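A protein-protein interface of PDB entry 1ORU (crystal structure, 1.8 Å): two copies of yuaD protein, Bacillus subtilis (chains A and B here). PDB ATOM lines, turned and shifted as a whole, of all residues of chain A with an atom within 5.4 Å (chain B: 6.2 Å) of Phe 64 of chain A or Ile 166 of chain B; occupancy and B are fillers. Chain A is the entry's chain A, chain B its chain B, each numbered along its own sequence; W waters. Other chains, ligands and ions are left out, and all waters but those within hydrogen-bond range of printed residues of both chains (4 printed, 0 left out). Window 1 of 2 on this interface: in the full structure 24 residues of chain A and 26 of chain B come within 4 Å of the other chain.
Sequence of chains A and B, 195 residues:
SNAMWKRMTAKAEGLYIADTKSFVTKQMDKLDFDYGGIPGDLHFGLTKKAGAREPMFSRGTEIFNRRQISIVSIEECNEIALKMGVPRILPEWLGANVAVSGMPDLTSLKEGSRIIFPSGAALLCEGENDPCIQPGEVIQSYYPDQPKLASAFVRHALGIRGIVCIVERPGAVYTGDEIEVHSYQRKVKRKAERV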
ATOM      1  N   LEU A  46      21.654 -14.124 -18.432  1.00  0.00           N
ATOM      2  CA  LEU A  46      22.597 -14.157 -17.321  1.00  0.00           C
ATOM      3  C   LEU A  46      22.300 -12.992 -16.384  1.00  0.00           C
ATOM      4  O   LEU A  46      22.441 -13.106 -15.168  1.00  0.00           O
ATOM      5  CB  LEU A  46      24.032 -14.029 -17.852  1.00  0.00           C
ATOM      6  CG  LEU A  46      25.163 -13.811 -16.839  1.00  0.00           C
ATOM      7  CD1 LEU A  46      25.340 -15.061 -15.991  1.00  0.00           C
ATOM      8  CD2 LEU A  46      26.457 -13.477 -17.571  1.00  0.00           C
ATOM      9  N   THR A  47      21.879 -11.869 -16.958  1.00  0.00           N
ATOM     10  CA  THR A  47      21.598 -10.685 -16.166  1.00  0.00           C
ATOM     11  C   THR A  47      20.203 -10.114 -16.378  1.00  0.00           C
ATOM     12  O   THR A  47      19.467 -10.532 -17.275  1.00  0.00           O
ATOM     13  CB  THR A  47      22.609  -9.571 -16.478  1.00  0.00           C
ATOM     14  OG1 THR A  47      22.440  -9.146 -17.837  1.00  0.00           O
ATOM     15  CG2 THR A  47      24.038 -10.075 -16.291  1.00  0.00           C
ATOM     16  N   LYS A  48      19.856  -9.150 -15.534  1.00  0.00           N
ATOM     17  CA  LYS A  48      18.575  -8.464 -15.604  1.00  0.00           C
ATOM     18  C   LYS A  48      18.777  -7.076 -15.006  1.00  0.00           C
ATOM     19  O   LYS A  48      19.806  -6.805 -14.383  1.00  0.00           O
ATOM     20  CB  LYS A  48      17.509  -9.208 -14.797  1.00  0.00           C
ATOM     21  CG  LYS A  48      17.784  -9.260 -13.303  1.00  0.00           C
ATOM     22  CD  LYS A  48      16.524  -9.578 -12.517  1.00  0.00           C
ATOM     23  CE  LYS A  48      15.531  -8.426 -12.613  1.00  0.00           C
ATOM     24  NZ  LYS A  48      14.296  -8.672 -11.829  1.00  0.00           N
ATOM     25  N   GLU A  62      22.407  -3.281 -13.680  1.00  0.00           N
ATOM     26  CA  GLU A  62      22.527  -4.634 -14.211  1.00  0.00           C
ATOM     27  C   GLU A  62      23.022  -5.573 -13.116  1.00  0.00           C
ATOM     28  O   GLU A  62      24.076  -5.348 -12.516  1.00  0.00           O
ATOM     29  CB  GLU A  62      23.489  -4.686 -15.401  1.00  0.00           C
ATOM     30  CG  GLU A  62      23.585  -6.074 -16.026  1.00  0.00           C
ATOM     31  CD  GLU A  62      24.411  -6.105 -17.298  1.00  0.00           C
ATOM     32  OE1 GLU A  62      25.614  -5.787 -17.245  1.00  0.00           O
ATOM     33  OE2 GLU A  62      23.852  -6.455 -18.360  1.00  0.00           O
ATOM     34  N   ILE A  63      22.242  -6.618 -12.859  1.00  0.00           N
ATOM     35  CA  ILE A  63      22.573  -7.603 -11.837  1.00  0.00           C
ATOM     36  C   ILE A  63      22.325  -8.999 -12.383  1.00  0.00           C
ATOM     37  O   ILE A  63      21.730  -9.167 -13.449  1.00  0.00           O
ATOM     38  CB  ILE A  63      21.703  -7.430 -10.567  1.00  0.00           C
ATOM     39  CG1 ILE A  63      20.219  -7.554 -10.927  1.00  0.00           C
ATOM     40  CG2 ILE A  63      21.997  -6.087  -9.903  1.00  0.00           C
ATOM     41  CD1 ILE A  63      19.280  -7.368  -9.756  1.00  0.00           C
ATOM     42  N   PHE A  64      22.786  -9.999 -11.643  1.00  0.00           N
ATOM     43  CA  PHE A  64      22.601 -11.384 -12.042  1.00  0.00           C
ATOM     44  C   PHE A  64      21.102 -11.690 -12.102  1.00  0.00           C
ATOM     45  O   PHE A  64      20.338 -11.217 -11.264  1.00  0.00           O
ATOM     46  CB  PHE A  64      23.263 -12.314 -11.027  1.00  0.00           C
ATOM     47  CG  PHE A  64      22.974 -13.757 -11.271  1.00  0.00           C
ATOM     48  CD1 PHE A  64      23.547 -14.418 -12.352  1.00  0.00           C
ATOM     49  CD2 PHE A  64      22.094 -14.448 -10.445  1.00  0.00           C
ATOM     50  CE1 PHE A  64      23.247 -15.754 -12.612  1.00  0.00           C
ATOM     51  CE2 PHE A  64      21.784 -15.784 -10.697  1.00  0.00           C
ATOM     52  CZ  PHE A  64      22.363 -16.437 -11.783  1.00  0.00           C
ATOM     53  N   ASN A  65      20.692 -12.489 -13.083  1.00  0.00           N
ATOM     54  CA  ASN A  65      19.282 -12.845 -13.232  1.00  0.00           C
ATOM     55  C   ASN A  65      18.914 -14.074 -12.405  1.00  0.00           C
ATOM     56  O   ASN A  65      19.061 -15.218 -12.839  1.00  0.00           O
ATOM     57  CB  ASN A  65      18.945 -13.075 -14.705  1.00  0.00           C
ATOM     58  CG  ASN A  65      17.498 -13.486 -14.916  1.00  0.00           C
ATOM     59  OD1 ASN A  65      16.633 -13.209 -14.083  1.00  0.00           O
ATOM     60  ND2 ASN A  65      17.228 -14.141 -16.036  1.00  0.00           N
ATOM     61  N   ARG A  66      18.415 -13.807 -11.209  1.00  0.00           N
ATOM     62  CA  ARG A  66      18.020 -14.826 -10.251  1.00  0.00           C
ATOM     63  C   ARG A  66      16.625 -15.399 -10.524  1.00  0.00           C
ATOM     64  O   ARG A  66      16.329 -16.538 -10.168  1.00  0.00           O
ATOM     65  CB  ARG A  66      18.053 -14.194  -8.867  1.00  0.00           C
ATOM     66  CG  ARG A  66      17.673 -15.092  -7.739  1.00  0.00           C
ATOM     67  CD  ARG A  66      17.403 -14.263  -6.501  1.00  0.00           C
ATOM     68  NE  ARG A  66      17.325 -15.112  -5.322  1.00  0.00           N
ATOM     69  CZ  ARG A  66      16.604 -14.834  -4.243  1.00  0.00           C
ATOM     70  NH1 ARG A  66      15.886 -13.720  -4.196  1.00  0.00           N
ATOM     71  NH2 ARG A  66      16.613 -15.667  -3.210  1.00  0.00           N
ATOM     72  N   GLN A  68      14.904 -16.653 -13.172  1.00  0.00           N
ATOM     73  CA  GLN A  68      14.899 -17.236 -14.512  1.00  0.00           C
ATOM     74  C   GLN A  68      13.635 -17.996 -14.880  1.00  0.00           C
ATOM     75  O   GLN A  68      13.183 -17.929 -16.018  1.00  0.00           O
ATOM     76  CB  GLN A  68      16.104 -18.164 -14.673  1.00  0.00           C
ATOM     77  CG  GLN A  68      17.428 -17.428 -14.681  1.00  0.00           C
ATOM     78  CD  GLN A  68      18.616 -18.363 -14.576  1.00  0.00           C
ATOM     79  OE1 GLN A  68      18.538 -19.528 -14.960  1.00  0.00           O
ATOM     80  NE2 GLN A  68      19.729 -17.850 -14.067  1.00  0.00           N
ATOM     81  N   ILE A 166      16.314 -20.848 -10.674  1.00  0.00           N
ATOM     82  CA  ILE A 166      17.431 -20.668 -11.594  1.00  0.00           C
ATOM     83  C   ILE A 166      17.538 -22.036 -12.265  1.00  0.00           C
ATOM     84  O   ILE A 166      17.194 -23.044 -11.647  1.00  0.00           O
ATOM     85  CB  ILE A 166      18.745 -20.388 -10.826  1.00  0.00           C
ATOM     86  CG1 ILE A 166      18.815 -18.911 -10.436  1.00  0.00           C
ATOM     87  CG2 ILE A 166      19.948 -20.813 -11.657  1.00  0.00           C
ATOM     88  CD1 ILE A 166      19.973 -18.602  -9.482  1.00  0.00           C
ATOM     89  N   TYR B  35      30.511 -12.292 -12.503  1.00  0.00           N
ATOM     90  CA  TYR B  35      29.553 -13.387 -12.509  1.00  0.00           C
ATOM     91  C   TYR B  35      30.339 -14.700 -12.576  1.00  0.00           C
ATOM     92  O   TYR B  35      31.140 -14.911 -13.488  1.00  0.00           O
ATOM     93  CB  TYR B  35      28.605 -13.242 -13.702  1.00  0.00           C
ATOM     94  CG  TYR B  35      27.837 -11.938 -13.692  1.00  0.00           C
ATOM     95  CD1 TYR B  35      26.918 -11.655 -12.680  1.00  0.00           C
ATOM     96  CD2 TYR B  35      28.038 -10.979 -14.687  1.00  0.00           C
ATOM     97  CE1 TYR B  35      26.216 -10.445 -12.658  1.00  0.00           C
ATOM     98  CE2 TYR B  35      27.340  -9.768 -14.676  1.00  0.00           C
ATOM     99  CZ  TYR B  35      26.435  -9.509 -13.660  1.00  0.00           C
ATOM    100  OH  TYR B  35      25.752  -8.310 -13.634  1.00  0.00           O
ATOM    101  N   LEU B  46      30.543 -20.252 -14.199  1.00  0.00           N
ATOM    102  CA  LEU B  46      29.092 -20.271 -14.171  1.00  0.00           C
ATOM    103  C   LEU B  46      28.593 -21.681 -13.865  1.00  0.00           C
ATOM    104  O   LEU B  46      27.437 -21.865 -13.476  1.00  0.00           O
ATOM    105  CB  LEU B  46      28.529 -19.755 -15.494  1.00  0.00           C
ATOM    106  CG  LEU B  46      28.834 -18.269 -15.722  1.00  0.00           C
ATOM    107  CD1 LEU B  46      28.325 -17.839 -17.083  1.00  0.00           C
ATOM    108  CD2 LEU B  46      28.188 -17.449 -14.617  1.00  0.00           C
ATOM    109  N   PHE B  64      24.789 -25.690 -12.529  1.00  0.00           N
ATOM    110  CA  PHE B  64      25.002 -24.280 -12.229  1.00  0.00           C
ATOM    111  C   PHE B  64      25.842 -24.175 -10.954  1.00  0.00           C
ATOM    112  O   PHE B  64      25.711 -24.994 -10.044  1.00  0.00           O
ATOM    113  CB  PHE B  64      23.663 -23.567 -12.020  1.00  0.00           C
ATOM    114  CG  PHE B  64      23.804 -22.158 -11.498  1.00  0.00           C
ATOM    115  CD1 PHE B  64      24.249 -21.132 -12.328  1.00  0.00           C
ATOM    116  CD2 PHE B  64      23.533 -21.868 -10.165  1.00  0.00           C
ATOM    117  CE1 PHE B  64      24.424 -19.833 -11.830  1.00  0.00           C
ATOM    118  CE2 PHE B  64      23.703 -20.578  -9.662  1.00  0.00           C
ATOM    119  CZ  PHE B  64      24.151 -19.561 -10.498  1.00  0.00           C
ATOM    120  N   ASN B  65      26.699 -23.163 -10.886  1.00  0.00           N
ATOM    121  CA  ASN B  65      27.562 -22.977  -9.721  1.00  0.00           C
ATOM    122  C   ASN B  65      26.972 -21.972  -8.733  1.00  0.00           C
ATOM    123  O   ASN B  65      27.147 -20.760  -8.892  1.00  0.00           O
ATOM    124  CB  ASN B  65      28.952 -22.516 -10.190  1.00  0.00           C
ATOM    125  CG  ASN B  65      29.943 -22.365  -9.044  1.00  0.00           C
ATOM    126  OD1 ASN B  65      29.750 -22.917  -7.963  1.00  0.00           O
ATOM    127  ND2 ASN B  65      31.019 -21.626  -9.289  1.00  0.00           N
ATOM    128  N   ARG B  66      26.261 -22.466  -7.718  1.00  0.00           N
ATOM    129  CA  ARG B  66      25.665 -21.565  -6.733  1.00  0.00           C
ATOM    130  C   ARG B  66      26.637 -21.314  -5.586  1.00  0.00           C
ATOM    131  O   ARG B  66      26.361 -20.512  -4.704  1.00  0.00           O
ATOM    132  CB  ARG B  66      24.344 -22.135  -6.185  1.00  0.00           C
ATOM    133  CG  ARG B  66      24.489 -23.292  -5.214  1.00  0.00           C
ATOM    134  CD  ARG B  66      23.140 -23.926  -4.840  1.00  0.00           C
ATOM    135  NE  ARG B  66      22.287 -23.094  -3.988  1.00  0.00           N
ATOM    136  CZ  ARG B  66      21.795 -23.484  -2.811  1.00  0.00           C
ATOM    137  NH1 ARG B  66      22.082 -24.688  -2.332  1.00  0.00           N
ATOM    138  NH2 ARG B  66      20.979 -22.693  -2.130  1.00  0.00           N
ATOM    139  N   ARG B  67      27.783 -21.994  -5.622  1.00  0.00           N
ATOM    140  CA  ARG B  67      28.810 -21.875  -4.587  1.00  0.00           C
ATOM    141  C   ARG B  67      30.031 -21.138  -5.137  1.00  0.00           C
ATOM    142  O   ARG B  67      31.153 -21.660  -5.125  1.00  0.00           O
ATOM    143  CB  ARG B  67      29.221 -23.267  -4.102  1.00  0.00           C
ATOM    144  CG  ARG B  67      28.119 -24.057  -3.379  1.00  0.00           C
ATOM    145  CD  ARG B  67      28.557 -25.510  -3.126  1.00  0.00           C
ATOM    146  NE  ARG B  67      29.767 -25.582  -2.309  1.00  0.00           N
ATOM    147  CZ  ARG B  67      29.796 -25.432  -0.986  1.00  0.00           C
ATOM    148  NH1 ARG B  67      28.679 -25.211  -0.309  1.00  0.00           N
ATOM    149  NH2 ARG B  67      30.953 -25.475  -0.340  1.00  0.00           N
ATOM    150  N   GLN B  68      29.804 -19.918  -5.602  1.00  0.00           N
ATOM    151  CA  GLN B  68      30.857 -19.101  -6.191  1.00  0.00           C
ATOM    152  C   GLN B  68      31.796 -18.440  -5.186  1.00  0.00           C
ATOM    153  O   GLN B  68      32.997 -18.354  -5.423  1.00  0.00           O
ATOM    154  CB  GLN B  68      30.223 -18.024  -7.075  1.00  0.00           C
ATOM    155  CG  GLN B  68      29.432 -18.572  -8.257  1.00  0.00           C
ATOM    156  CD  GLN B  68      28.682 -17.487  -9.002  1.00  0.00           C
ATOM    157  OE1 GLN B  68      28.977 -16.294  -8.855  1.00  0.00           O
ATOM    158  NE2 GLN B  68      27.711 -17.891  -9.813  1.00  0.00           N
ATOM    159  N   ILE B  69      31.241 -17.966  -4.075  1.00  0.00           N
ATOM    160  CA  ILE B  69      32.020 -17.293  -3.040  1.00  0.00           C
ATOM    161  C   ILE B  69      31.646 -17.872  -1.678  1.00  0.00           C
ATOM    162  O   ILE B  69      30.465 -18.091  -1.399  1.00  0.00           O
ATOM    163  CB  ILE B  69      31.697 -15.766  -3.018  1.00  0.00           C
ATOM    164  CG1 ILE B  69      31.953 -15.140  -4.395  1.00  0.00           C
ATOM    165  CG2 ILE B  69      32.514 -15.062  -1.942  1.00  0.00           C
ATOM    166  CD1 ILE B  69      33.405 -14.984  -4.761  1.00  0.00           C
ATOM    167  N   ALA B 122      28.273  -6.886  -5.319  1.00  0.00           N
ATOM    168  CA  ALA B 122      27.283  -7.478  -4.428  1.00  0.00           C
ATOM    169  C   ALA B 122      27.216  -8.994  -4.498  1.00  0.00           C
ATOM    170  O   ALA B 122      27.414  -9.590  -5.558  1.00  0.00           O
ATOM    171  CB  ALA B 122      25.905  -6.889  -4.717  1.00  0.00           C
ATOM    172  N   LEU B 123      26.922  -9.605  -3.354  1.00  0.00           N
ATOM    173  CA  LEU B 123      26.812 -11.050  -3.252  1.00  0.00           C
ATOM    174  C   LEU B 123      25.399 -11.437  -2.829  1.00  0.00           C
ATOM    175  O   LEU B 123      24.801 -10.779  -1.970  1.00  0.00           O
ATOM    176  CB  LEU B 123      27.817 -11.580  -2.224  1.00  0.00           C
ATOM    177  CG  LEU B 123      29.298 -11.289  -2.488  1.00  0.00           C
ATOM    178  CD1 LEU B 123      30.147 -11.931  -1.395  1.00  0.00           C
ATOM    179  CD2 LEU B 123      29.699 -11.838  -3.862  1.00  0.00           C
ATOM    180  N   LEU B 124      24.869 -12.491  -3.445  1.00  0.00           N
ATOM    181  CA  LEU B 124      23.539 -13.006  -3.121  1.00  0.00           C
ATOM    182  C   LEU B 124      23.733 -14.272  -2.284  1.00  0.00           C
ATOM    183  O   LEU B 124      24.343 -15.239  -2.742  1.00  0.00           O
ATOM    184  CB  LEU B 124      22.761 -13.355  -4.395  1.00  0.00           C
ATOM    185  CG  LEU B 124      21.484 -14.183  -4.185  1.00  0.00           C
ATOM    186  CD1 LEU B 124      20.447 -13.352  -3.445  1.00  0.00           C
ATOM    187  CD2 LEU B 124      20.935 -14.648  -5.524  1.00  0.00           C
ATOM    188  N   CYS B 125      23.208 -14.271  -1.064  1.00  0.00           N
ATOM    189  CA  CYS B 125      23.353 -15.419  -0.178  1.00  0.00           C
ATOM    190  C   CYS B 125      22.633 -16.665  -0.677  1.00  0.00           C
ATOM    191  O   CYS B 125      21.439 -16.621  -1.002  1.00  0.00           O
ATOM    192  CB  CYS B 125      22.841 -15.070   1.223  1.00  0.00           C
ATOM    193  SG  CYS B 125      23.111 -16.375   2.451  1.00  0.00           S
ATOM    194  N   GLU B 126      23.370 -17.773  -0.735  1.00  0.00           N
ATOM    195  CA  GLU B 126      22.830 -19.058  -1.161  1.00  0.00           C
ATOM    196  C   GLU B 126      22.831 -20.043   0.006  1.00  0.00           C
ATOM    197  O   GLU B 126      22.902 -21.263  -0.185  1.00  0.00           O
ATOM    198  CB  GLU B 126      23.633 -19.632  -2.331  1.00  0.00           C
ATOM    199  CG  GLU B 126      23.350 -18.966  -3.672  1.00  0.00           C
ATOM    200  CD  GLU B 126      21.933 -19.211  -4.179  1.00  0.00           C
ATOM    201  OE1 GLU B 126      21.427 -20.343  -4.032  1.00  0.00           O
ATOM    202  OE2 GLU B 126      21.325 -18.271  -4.738  1.00  0.00           O
ATOM    203  N   VAL B 164      27.613 -19.589   1.563  1.00  0.00           N
ATOM    204  CA  VAL B 164      28.107 -19.549   0.191  1.00  0.00           C
ATOM    205  C   VAL B 164      27.208 -18.556  -0.535  1.00  0.00           C
ATOM    206  O   VAL B 164      26.034 -18.400  -0.182  1.00  0.00           O
ATOM    207  CB  VAL B 164      28.031 -20.921  -0.519  1.00  0.00           C
ATOM    208  CG1 VAL B 164      29.165 -21.816  -0.037  1.00  0.00           C
ATOM    209  CG2 VAL B 164      26.681 -21.576  -0.260  1.00  0.00           C
ATOM    210  N   CYS B 165      27.758 -17.881  -1.539  1.00  0.00           N
ATOM    211  CA  CYS B 165      27.003 -16.883  -2.294  1.00  0.00           C
ATOM    212  C   CYS B 165      27.330 -16.936  -3.772  1.00  0.00           C
ATOM    213  O   CYS B 165      28.290 -17.575  -4.187  1.00  0.00           O
ATOM    214  CB  CYS B 165      27.356 -15.464  -1.834  1.00  0.00           C
ATOM    215  SG  CYS B 165      27.155 -15.063  -0.090  1.00  0.00           S
ATOM    216  N   ILE B 166      26.516 -16.257  -4.568  1.00  0.00           N
ATOM    217  CA  ILE B 166      26.803 -16.149  -5.990  1.00  0.00           C
ATOM    218  C   ILE B 166      27.015 -14.649  -6.158  1.00  0.00           C
ATOM    219  O   ILE B 166      26.532 -13.856  -5.347  1.00  0.00           O
ATOM    220  CB  ILE B 166      25.626 -16.617  -6.888  1.00  0.00           C
ATOM    221  CG1 ILE B 166      24.361 -15.833  -6.562  1.00  0.00           C
ATOM    222  CG2 ILE B 166      25.401 -18.109  -6.715  1.00  0.00           C
ATOM    223  CD1 ILE B 166      23.194 -16.160  -7.475  1.00  0.00           C
ATOM    224  N   VAL B 167      27.761 -14.250  -7.176  1.00  0.00           N
ATOM    225  CA  VAL B 167      27.985 -12.833  -7.397  1.00  0.00           C
ATOM    226  C   VAL B 167      26.762 -12.252  -8.101  1.00  0.00           C
ATOM    227  O   VAL B 167      26.411 -12.690  -9.192  1.00  0.00           O
ATOM    228  CB  VAL B 167      29.237 -12.593  -8.259  1.00  0.00           C
ATOM    229  CG1 VAL B 167      29.333 -11.116  -8.636  1.00  0.00           C
ATOM    230  CG2 VAL B 167      30.484 -13.029  -7.494  1.00  0.00           C
ATOM    231  N   GLU B 168      26.113 -11.278  -7.469  1.00  0.00           N
ATOM    232  CA  GLU B 168      24.928 -10.646  -8.045  1.00  0.00           C
ATOM    233  C   GLU B 168      25.279  -9.383  -8.833  1.00  0.00           C
ATOM    234  O   GLU B 168      24.560  -9.003  -9.757  1.00  0.00           O
ATOM    235  CB  GLU B 168      23.904 -10.331  -6.950  1.00  0.00           C
ATOM    236  CG  GLU B 168      22.626  -9.693  -7.478  1.00  0.00           C
ATOM    237  CD  GLU B 168      21.482  -9.756  -6.489  1.00  0.00           C
ATOM    238  OE1 GLU B 168      21.744  -9.727  -5.267  1.00  0.00           O
ATOM    239  OE2 GLU B 168      20.315  -9.822  -6.936  1.00  0.00           O
ATOM    240  N   ARG B 169      26.377  -8.727  -8.462  1.00  0.00           N
ATOM    241  CA  ARG B 169      26.835  -7.543  -9.194  1.00  0.00           C
ATOM    242  C   ARG B 169      28.355  -7.484  -9.135  1.00  0.00           C
ATOM    243  O   ARG B 169      28.940  -7.501  -8.054  1.00  0.00           O
ATOM    244  CB  ARG B 169      26.257  -6.248  -8.618  1.00  0.00           C
ATOM    245  CG  ARG B 169      26.512  -5.069  -9.553  1.00  0.00           C
ATOM    246  CD  ARG B 169      26.166  -3.726  -8.959  1.00  0.00           C
ATOM    247  NE  ARG B 169      26.381  -2.666  -9.940  1.00  0.00           N
ATOM    248  CZ  ARG B 169      26.319  -1.367  -9.668  1.00  0.00           C
ATOM    249  NH1 ARG B 169      26.045  -0.959  -8.433  1.00  0.00           N
ATOM    250  NH2 ARG B 169      26.530  -0.475 -10.631  1.00  0.00           N
ATOM    251  N   PRO B 170      29.017  -7.428 -10.304  1.00  0.00           N
ATOM    252  CA  PRO B 170      30.481  -7.370 -10.387  1.00  0.00           C
ATOM    253  C   PRO B 170      31.074  -6.129  -9.727  1.00  0.00           C
ATOM    254  O   PRO B 170      30.405  -5.104  -9.591  1.00  0.00           O
ATOM    255  CB  PRO B 170      30.744  -7.397 -11.894  1.00  0.00           C
ATOM    256  CG  PRO B 170      29.555  -8.128 -12.439  1.00  0.00           C
ATOM    257  CD  PRO B 170      28.427  -7.515 -11.650  1.00  0.00           C
HETATM  258  O   HOH W   1      19.269 -17.272  -2.714  1.00  0.00           O
HETATM  259  O   HOH W   2      26.138  -3.578 -12.855  1.00  0.00           O
HETATM  260  O   HOH W   3      26.742  -6.560 -15.180  1.00  0.00           O
HETATM  261  O   HOH W   4      18.902 -11.035  -8.828  1.00  0.00           O
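The backbone NH (N) of Phe 64 of chain A is in hydrogen-bond range of the backbone carbonyl oxygen (O) of Glu 168 of chain B, 2.8 Å away.
O of Leu 46 of chain A is in hydrogen-bond range of N of Asn 65 of chain A (2.8 Å). The side-chain hydroxyl of Thr 47 of chain A is in hydrogen-bond range of the side-chain carboxylate of Glu 62 of chain A, at 3.1 Å. O of Ile 63 of chain A lies within hydrogen-bond range of N of Lys 48 of chain A, 2.8 Å away. The backbone NH of Val 167 of chain B is in hydrogen-bond range of the side-chain amide oxygen of Gln 68 of chain B (2.9 Å). The backbone NH of Ala 122 of chain B is in hydrogen-bond range of the backbone carbonyl oxygen of Arg 169 of chain B, at 2.9 Å. The backbone NH (N) of Leu 124 of chain B lies within hydrogen-bond range of the backbone carbonyl oxygen (O) of Ile 166 of chain B (2.9 Å).
Leu 46 of chain B touches Leu 46 of chain A. Tyr 35 of chain B touches Glu 62 of chain A (OH to O, 3.6 Å). Glu 62 of chain A touches Arg 169 of chain B. Tyr 35 of chain B touches Ile 63 of chain A. CA of Ile 63 of chain A touches O of Glu 168 of chain B (3.2 Å). Phe 64 of chain A touches Tyr 35 of chain B. Phe 64 of chain A touches Phe 64 of chain B. CE2 of Phe 64 of chain A touches CD1 of Ile 166 of chain B, 3.5 Å away. Phe 64 of chain A touches Val 167 of chain B. Arg 66 of chain A touches Leu 124 of chain B (NE to CD2, 3.6 Å).
Of chain B, only Tyr 35 (3.6 Å), Phe 64 (3.8 Å), Ile 166 (3.5 Å), Val 167 (3.7 Å) and Glu 168 (2.8 Å) come within 4 Å of Phe 64 of chain A. Printed residues of chain B within 4 Å of Thr 47 of chain A: Tyr 35 (3.6 Å). Printed residues of chain B within 4 Å of Arg 66 of chain A: Leu 124 (3.6 Å). Leu 123 of chain B touches none of the printed residues of chain A.
Of the 10 printed residues of chain A, 6 touch a printed residue of chain B. Hydrophobic or aromatic side chains of chain A that line the printed part of chain B: Leu 46, Ile 63 and Phe 64. Hydrophobic or aromatic side chains of chain B that line the printed part of chain A: Tyr 35, Leu 46, Phe 64, Leu 124 and Ile 166. Among the printed residues, no Asp or Glu carboxylate lies within 4 Å of a Lys or Arg side-chain nitrogen of the other chain.
Leu 46 of chain A touches its own counterpart, Leu 46 of chain B. Phe 64 of chain B touches its own counterpart, Phe 64 of chain A. Phe 64 of chain A touches Ile 166 of chain B, but with the chains exchanged Ile 166 of chain A does not touch Phe 64 of chain B (4.02 Å). Positions printed for both chains: 46, 64, 65, 66, 68 and 166. Of the 12 pairs that touch across the chains among the printed residues, 2 have their exchanged pair printed and touching as well.
Water W3 lies within hydrogen-bond range of the side-chain carboxylate (OE1) of Glu 62 of chain A (2.5 Å) and the side-chain hydroxyl (OH) of Tyr 35 of chain B (2.5 Å). Water W4 bridges OE2 of Glu 168 of chain B (2.7 Å) and O of Phe 64 of chain A (2.8 Å). Water W2 bridges the backbone carbonyl oxygen of Glu 62 of chain A and the guanidinium group of Arg 169 of chain B. Water W1 lies within hydrogen-bond range of O of Cys 125 of chain B (2.8 Å), OE2 of Glu 126 of chain B (3.1 Å) and NH2 of Arg 66 of chain A (3.1 Å).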
